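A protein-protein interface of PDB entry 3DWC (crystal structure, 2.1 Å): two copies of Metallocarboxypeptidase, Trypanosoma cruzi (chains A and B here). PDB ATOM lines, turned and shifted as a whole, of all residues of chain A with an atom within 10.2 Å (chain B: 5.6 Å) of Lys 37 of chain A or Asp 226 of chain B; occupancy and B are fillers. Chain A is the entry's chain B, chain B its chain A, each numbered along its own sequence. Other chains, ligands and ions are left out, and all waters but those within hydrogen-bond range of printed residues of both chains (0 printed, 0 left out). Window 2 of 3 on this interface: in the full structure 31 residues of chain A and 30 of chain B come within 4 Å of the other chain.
Ser 30 of chain A touches none of the printed residues of chain B. Printed residues of chain B within 4 Å of CSX 36 of chain A: Asp 228. Lys 37 of chain A touches just these residues of chain B: Asp 226, Asp 228 and Glu 245. Printed residues of chain B within 4 Å of Ala 41 of chain A: Glu 245. No residue of chain A comes within 4 Å of Phe 225 of chain B. Of the printed residues of chain A, Asp 226 of chain B touches Lys 37 (2.8 Å). Printed residues of chain A within 4 Å of Asp 228 of chain B: Pro 35 (3.2 Å), CSX 36 (3.4 Å) and Lys 37 (2.9 Å). No residue of chain A comes within 4 Å of Gly 229 of chain B. Gly 230 of chain B touches one residue of chain A. Lys 273 of chain B touches none of the printed residues of chain A. The nearest residue of chain B that does not touch Lys 37 of chain A is Gly 229 of chain B (4.3 Å). The nearest residue of chain A that does not touch Asp 226 of chain B is Pro 35 of chain A (6.3 Å).
Printed residues of chain A that touch a printed residue of chain B: Pro 35, CSX 36, Lys 37, Gly 38 and Ala 41. Hydrophobic or aromatic side chains of chain A within 4 Å of the printed part of chain B: Pro 35 and Ala 41. Of the 10 printed residues of chain B, 5 touch a printed residue of chain A. Among the printed residues, 9 pairs touch across the chains. Among the printed residues, Asp or Glu carboxylates within 4 Å of a Lys or Arg side-chain nitrogen of the other chain: Lys 37 of chain A with Asp 226 of chain B.
NZ of Lys 37 of chain A is in salt-bridge range of OD2 of Asp 226 of chain B (2.8 Å). The backbone carbonyl oxygen of Asp 228 of chain B lies within hydrogen-bond range of N of CSX 36 of chain A. The backbone carbonyl oxygen (O) of Asp 228 of chain B is in hydrogen-bond range of the backbone NH (N) of Lys 37 of chain A, at 2.9 Å.
OD1 of Asp 226 of chain B is in hydrogen-bond range of N of Asp 228 of chain B (2.9 Å). The backbone NH (N) of Asp 226 of chain B is in hydrogen-bond range of the side-chain amide oxygen (OE1) of Gln 276 of chain B (3.0 Å).
O of Phe 227 of chain B touches CB of Pro 35 of chain A (3.8 Å). Pro 35 of chain A touches Asp 228 of chain B (CB to O, 3.2 Å). N of Gly 230 of chain B touches CG of Pro 35 of chain A, 3.5 Å away. C of Lys 37 of chain A touches O of Glu 245 of chain B, at 3.9 Å. CA of Gly 38 of chain A touches O of Glu 245 of chain B, at 3.7 Å. Ala 41 of chain A touches Glu 245 of chain B.
No position is printed for both chains. Of the 9 pairs that touch across the chains among the printed residues, none has its exchanged pair printed and touching as well.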
ATOM      1  N   SER A  30      13.579  -8.539 -16.929  1.00  0.00           N
ATOM      2  CA  SER A  30      14.812  -8.874 -16.206  1.00  0.00           C
ATOM      3  C   SER A  30      14.764  -8.329 -14.770  1.00  0.00           C
ATOM      4  O   SER A  30      15.388  -8.876 -13.896  1.00  0.00           O
ATOM      5  CB  SER A  30      16.077  -8.357 -16.922  1.00  0.00           C
ATOM      6  OG  SER A  30      16.020  -6.943 -16.938  1.00  0.00           O
ATOM      7  N   MET A  33      10.341 -10.293 -13.367  1.00  0.00           N
ATOM      8  CA  MET A  33       9.906 -11.687 -13.415  1.00  0.00           C
ATOM      9  C   MET A  33      11.057 -12.663 -13.516  1.00  0.00           C
ATOM     10  O   MET A  33      10.909 -13.830 -13.141  1.00  0.00           O
ATOM     11  CB  MET A  33       8.986 -11.915 -14.628  1.00  0.00           C
ATOM     12  CG  MET A  33       7.747 -11.028 -14.699  1.00  0.00           C
ATOM     13  SD  MET A  33       6.792 -11.292 -13.181  1.00  0.00           S
ATOM     14  CE  MET A  33       5.909  -9.788 -13.037  1.00  0.00           C
ATOM     15  N   MET A  34      12.185 -12.230 -14.079  1.00  0.00           N
ATOM     16  CA  MET A  34      13.220 -13.192 -14.494  1.00  0.00           C
ATOM     17  C   MET A  34      13.923 -13.865 -13.316  1.00  0.00           C
ATOM     18  O   MET A  34      14.448 -13.193 -12.458  1.00  0.00           O
ATOM     19  CB  MET A  34      14.256 -12.493 -15.348  1.00  0.00           C
ATOM     20  CG  MET A  34      15.376 -13.401 -15.868  1.00  0.00           C
ATOM     21  SD  MET A  34      16.724 -12.408 -16.531  1.00  0.00           S
ATOM     22  CE  MET A  34      17.699 -12.107 -15.029  1.00  0.00           C
ATOM     23  N   PRO A  35      13.942 -15.186 -13.265  1.00  0.00           N
ATOM     24  CA  PRO A  35      14.747 -15.789 -12.228  1.00  0.00           C
ATOM     25  C   PRO A  35      16.242 -15.686 -12.487  1.00  0.00           C
ATOM     26  O   PRO A  35      16.646 -15.589 -13.636  1.00  0.00           O
ATOM     27  CB  PRO A  35      14.361 -17.267 -12.307  1.00  0.00           C
ATOM     28  CG  PRO A  35      13.899 -17.486 -13.622  1.00  0.00           C
ATOM     29  CD  PRO A  35      13.263 -16.205 -14.083  1.00  0.00           C
ATOM     30  N   CSX A  36      17.069 -15.897 -11.449  1.00  0.00           N
ATOM     31  CA  CSX A  36      18.478 -15.505 -11.509  1.00  0.00           C
ATOM     32  CB  CSX A  36      19.161 -15.438 -10.109  1.00  0.00           C
ATOM     33  SG  CSX A  36      19.377 -16.926  -9.395  1.00  0.00           S
ATOM     34  C   CSX A  36      19.300 -16.239 -12.543  1.00  0.00           C
ATOM     35  O   CSX A  36      20.142 -15.634 -13.192  1.00  0.00           O
ATOM     36  OD  CSX A  36      20.908 -17.939  -9.588  1.00  0.00           O
ATOM     37  N   LYS A  37      19.084 -17.525 -12.730  1.00  0.00           N
ATOM     38  CA  LYS A  37      19.827 -18.255 -13.741  1.00  0.00           C
ATOM     39  C   LYS A  37      19.521 -17.937 -15.226  1.00  0.00           C
ATOM     40  O   LYS A  37      20.243 -18.383 -16.094  1.00  0.00           O
ATOM     41  CB  LYS A  37      19.701 -19.755 -13.509  1.00  0.00           C
ATOM     42  CG  LYS A  37      20.433 -20.275 -12.274  1.00  0.00           C
ATOM     43  CD  LYS A  37      20.121 -21.731 -12.165  1.00  0.00           C
ATOM     44  CE  LYS A  37      20.598 -22.351 -10.941  1.00  0.00           C
ATOM     45  NZ  LYS A  37      20.655 -23.852 -11.068  1.00  0.00           N
ATOM     46  N   GLY A  38      18.467 -17.197 -15.511  1.00  0.00           N
ATOM     47  CA  GLY A  38      18.173 -16.743 -16.877  1.00  0.00           C
ATOM     48  C   GLY A  38      18.927 -15.518 -17.366  1.00  0.00           C
ATOM     49  O   GLY A  38      18.721 -15.053 -18.496  1.00  0.00           O
ATOM     50  N   SER A  39      19.752 -14.974 -16.465  1.00  0.00           N
ATOM     51  CA  SER A  39      20.449 -13.721 -16.618  1.00  0.00           C
ATOM     52  C   SER A  39      21.434 -13.670 -17.776  1.00  0.00           C
ATOM     53  O   SER A  39      21.403 -12.739 -18.555  1.00  0.00           O
ATOM     54  CB  SER A  39      21.184 -13.376 -15.313  1.00  0.00           C
ATOM     55  OG  SER A  39      21.670 -12.052 -15.414  1.00  0.00           O
ATOM     56  N   ASP A  40      22.344 -14.605 -17.866  1.00  0.00           N
ATOM     57  CA  ASP A  40      23.261 -14.626 -19.012  1.00  0.00           C
ATOM     58  C   ASP A  40      22.549 -14.732 -20.370  1.00  0.00           C
ATOM     59  O   ASP A  40      22.894 -14.001 -21.327  1.00  0.00           O
ATOM     60  CB  ASP A  40      24.245 -15.770 -18.877  1.00  0.00           C
ATOM     61  CG  ASP A  40      25.263 -15.547 -17.764  1.00  0.00           C
ATOM     62  OD1 ASP A  40      25.280 -14.467 -17.175  1.00  0.00           O
ATOM     63  OD2 ASP A  40      26.056 -16.469 -17.493  1.00  0.00           O
ATOM     64  N   ALA A  41      21.567 -15.642 -20.447  1.00  0.00           N
ATOM     65  CA  ALA A  41      20.752 -15.791 -21.667  1.00  0.00           C
ATOM     66  C   ALA A  41      20.072 -14.529 -22.042  1.00  0.00           C
ATOM     67  O   ALA A  41      20.019 -14.184 -23.219  1.00  0.00           O
ATOM     68  CB  ALA A  41      19.719 -16.910 -21.508  1.00  0.00           C
ATOM     69  N   ARG A  42      19.489 -13.841 -21.055  1.00  0.00           N
ATOM     70  CA  ARG A  42      18.802 -12.593 -21.308  1.00  0.00           C
ATOM     71  C   ARG A  42      19.759 -11.480 -21.764  1.00  0.00           C
ATOM     72  O   ARG A  42      19.409 -10.710 -22.650  1.00  0.00           O
ATOM     73  CB  ARG A  42      17.985 -12.140 -20.072  1.00  0.00           C
ATOM     74  CG  ARG A  42      17.411 -10.803 -20.097  1.00  0.00           C
ATOM     75  CD  ARG A  42      16.257 -10.621 -21.094  1.00  0.00           C
ATOM     76  NE  ARG A  42      15.298 -11.722 -20.953  1.00  0.00           N
ATOM     77  CZ  ARG A  42      14.390 -11.769 -19.982  1.00  0.00           C
ATOM     78  NH1 ARG A  42      14.265 -10.746 -19.154  1.00  0.00           N
ATOM     79  NH2 ARG A  42      13.590 -12.829 -19.857  1.00  0.00           N
ATOM     80  N   GLY A  43      20.951 -11.414 -21.180  1.00  0.00           N
ATOM     81  CA  GLY A  43      21.895 -10.322 -21.502  1.00  0.00           C
ATOM     82  C   GLY A  43      22.471 -10.559 -22.878  1.00  0.00           C
ATOM     83  O   GLY A  43      22.516  -9.633 -23.674  1.00  0.00           O
ATOM     84  N   ALA A  44      22.782 -11.814 -23.179  1.00  0.00           N
ATOM     85  CA  ALA A  44      23.233 -12.235 -24.532  1.00  0.00           C
ATOM     86  C   ALA A  44      22.190 -11.886 -25.623  1.00  0.00           C
ATOM     87  O   ALA A  44      22.511 -11.371 -26.722  1.00  0.00           O
ATOM     88  CB  ALA A  44      23.578 -13.696 -24.512  1.00  0.00           C
ATOM     89  N   LYS B 224      11.775 -31.627  -8.496  1.00  0.00           N
ATOM     90  CA  LYS B 224      13.020 -30.854  -8.408  1.00  0.00           C
ATOM     91  C   LYS B 224      13.144 -29.850  -9.534  1.00  0.00           C
ATOM     92  O   LYS B 224      14.183 -29.668 -10.093  1.00  0.00           O
ATOM     93  CB  LYS B 224      14.238 -31.777  -8.333  1.00  0.00           C
ATOM     94  CG  LYS B 224      13.980 -32.958  -7.433  1.00  0.00           C
ATOM     95  CD  LYS B 224      15.236 -33.490  -6.796  1.00  0.00           C
ATOM     96  CE  LYS B 224      14.942 -34.760  -5.962  1.00  0.00           C
ATOM     97  NZ  LYS B 224      14.129 -34.569  -4.708  1.00  0.00           N
ATOM     98  N   PHE B 225      12.025 -29.232  -9.894  1.00  0.00           N
ATOM     99  CA  PHE B 225      12.028 -28.087 -10.785  1.00  0.00           C
ATOM    100  C   PHE B 225      12.969 -27.009 -10.259  1.00  0.00           C
ATOM    101  O   PHE B 225      12.882 -26.648  -9.106  1.00  0.00           O
ATOM    102  CB  PHE B 225      10.610 -27.555 -10.887  1.00  0.00           C
ATOM    103  CG  PHE B 225      10.456 -26.433 -11.835  1.00  0.00           C
ATOM    104  CD1 PHE B 225      10.041 -26.655 -13.141  1.00  0.00           C
ATOM    105  CD2 PHE B 225      10.605 -25.128 -11.393  1.00  0.00           C
ATOM    106  CE1 PHE B 225       9.827 -25.603 -13.996  1.00  0.00           C
ATOM    107  CE2 PHE B 225      10.426 -24.067 -12.249  1.00  0.00           C
ATOM    108  CZ  PHE B 225      10.068 -24.300 -13.569  1.00  0.00           C
ATOM    109  N   ASP B 226      13.851 -26.500 -11.113  1.00  0.00           N
ATOM    110  CA  ASP B 226      14.784 -25.452 -10.699  1.00  0.00           C
ATOM    111  C   ASP B 226      14.097 -24.068 -10.790  1.00  0.00           C
ATOM    112  O   ASP B 226      13.996 -23.518 -11.833  1.00  0.00           O
ATOM    113  CB  ASP B 226      16.058 -25.496 -11.528  1.00  0.00           C
ATOM    114  CG  ASP B 226      17.063 -24.426 -11.103  1.00  0.00           C
ATOM    115  OD1 ASP B 226      16.843 -23.772 -10.052  1.00  0.00           O
ATOM    116  OD2 ASP B 226      18.030 -24.224 -11.855  1.00  0.00           O
ATOM    117  N   PHE B 227      13.612 -23.553  -9.664  1.00  0.00           N
ATOM    118  CA  PHE B 227      12.991 -22.241  -9.598  1.00  0.00           C
ATOM    119  C   PHE B 227      13.960 -21.077  -9.702  1.00  0.00           C
ATOM    120  O   PHE B 227      13.557 -19.936  -9.777  1.00  0.00           O
ATOM    121  CB  PHE B 227      12.137 -22.102  -8.331  1.00  0.00           C
ATOM    122  CG  PHE B 227      10.771 -22.751  -8.433  1.00  0.00           C
ATOM    123  CD1 PHE B 227      10.503 -23.943  -7.772  1.00  0.00           C
ATOM    124  CD2 PHE B 227       9.749 -22.156  -9.152  1.00  0.00           C
ATOM    125  CE1 PHE B 227       9.227 -24.528  -7.816  1.00  0.00           C
ATOM    126  CE2 PHE B 227       8.487 -22.760  -9.254  1.00  0.00           C
ATOM    127  CZ  PHE B 227       8.215 -23.925  -8.584  1.00  0.00           C
ATOM    128  N   ASP B 228      15.243 -21.331  -9.680  1.00  0.00           N
ATOM    129  CA  ASP B 228      16.203 -20.275 -10.079  1.00  0.00           C
ATOM    130  C   ASP B 228      16.302 -20.183 -11.628  1.00  0.00           C
ATOM    131  O   ASP B 228      16.853 -19.225 -12.162  1.00  0.00           O
ATOM    132  CB  ASP B 228      17.593 -20.549  -9.453  1.00  0.00           C
ATOM    133  CG  ASP B 228      17.629 -20.322  -7.937  1.00  0.00           C
ATOM    134  OD1 ASP B 228      18.497 -20.931  -7.267  1.00  0.00           O
ATOM    135  OD2 ASP B 228      16.844 -19.519  -7.414  1.00  0.00           O
ATOM    136  N   GLY B 229      15.750 -21.176 -12.321  1.00  0.00           N
ATOM    137  CA  GLY B 229      15.736 -21.279 -13.793  1.00  0.00           C
ATOM    138  C   GLY B 229      14.324 -21.487 -14.376  1.00  0.00           C
ATOM    139  O   GLY B 229      14.166 -22.094 -15.407  1.00  0.00           O
ATOM    140  N   GLY B 230      13.300 -20.941 -13.748  1.00  0.00           N
ATOM    141  CA  GLY B 230      11.920 -21.121 -14.242  1.00  0.00           C
ATOM    142  C   GLY B 230      10.874 -20.534 -13.348  1.00  0.00           C
ATOM    143  O   GLY B 230      11.212 -20.026 -12.314  1.00  0.00           O
ATOM    144  N   GLU B 245      16.948 -21.815 -20.247  1.00  0.00           N
ATOM    145  CA  GLU B 245      17.570 -21.222 -19.040  1.00  0.00           C
ATOM    146  C   GLU B 245      16.506 -20.605 -18.098  1.00  0.00           C
ATOM    147  O   GLU B 245      16.835 -20.148 -17.014  1.00  0.00           O
ATOM    148  CB  GLU B 245      18.554 -20.137 -19.448  1.00  0.00           C
ATOM    149  CG  GLU B 245      19.585 -20.524 -20.504  1.00  0.00           C
ATOM    150  CD  GLU B 245      19.154 -20.355 -21.964  1.00  0.00           C
ATOM    151  OE1 GLU B 245      20.052 -20.557 -22.806  1.00  0.00           O
ATOM    152  OE2 GLU B 245      17.960 -20.075 -22.307  1.00  0.00           O
ATOM    153  N   LYS B 273      11.280 -30.293 -17.180  1.00  0.00           N
ATOM    154  CA  LYS B 273      12.505 -31.039 -16.773  1.00  0.00           C
ATOM    155  C   LYS B 273      13.446 -31.368 -17.939  1.00  0.00           C
ATOM    156  O   LYS B 273      14.692 -31.368 -17.827  1.00  0.00           O
ATOM    157  CB  LYS B 273      12.124 -32.358 -16.092  1.00  0.00           C
ATOM    158  CG  LYS B 273      11.516 -32.271 -14.664  1.00  0.00           C
ATOM    159  CD  LYS B 273      12.368 -31.535 -13.663  1.00  0.00           C
ATOM    160  CE  LYS B 273      13.541 -32.355 -13.205  1.00  0.00           C
ATOM    161  NZ  LYS B 273      14.318 -31.577 -12.260  1.00  0.00           N
ATOM    162  N   GLN B 276      14.887 -27.953 -19.072  1.00  0.00           N
ATOM    163  CA  GLN B 276      15.894 -27.449 -18.096  1.00  0.00           C
ATOM    164  C   GLN B 276      17.178 -28.238 -18.136  1.00  0.00           C
ATOM    165  O   GLN B 276      18.192 -27.715 -17.747  1.00  0.00           O
ATOM    166  CB  GLN B 276      15.434 -27.428 -16.614  1.00  0.00           C
ATOM    167  CG  GLN B 276      14.245 -26.557 -16.363  1.00  0.00           C
ATOM    168  CD  GLN B 276      13.927 -26.293 -14.919  1.00  0.00           C
ATOM    169  OE1 GLN B 276      13.968 -27.206 -14.075  1.00  0.00           O
ATOM    170  NE2 GLN B 276      13.623 -25.019 -14.608  1.00  0.00           N
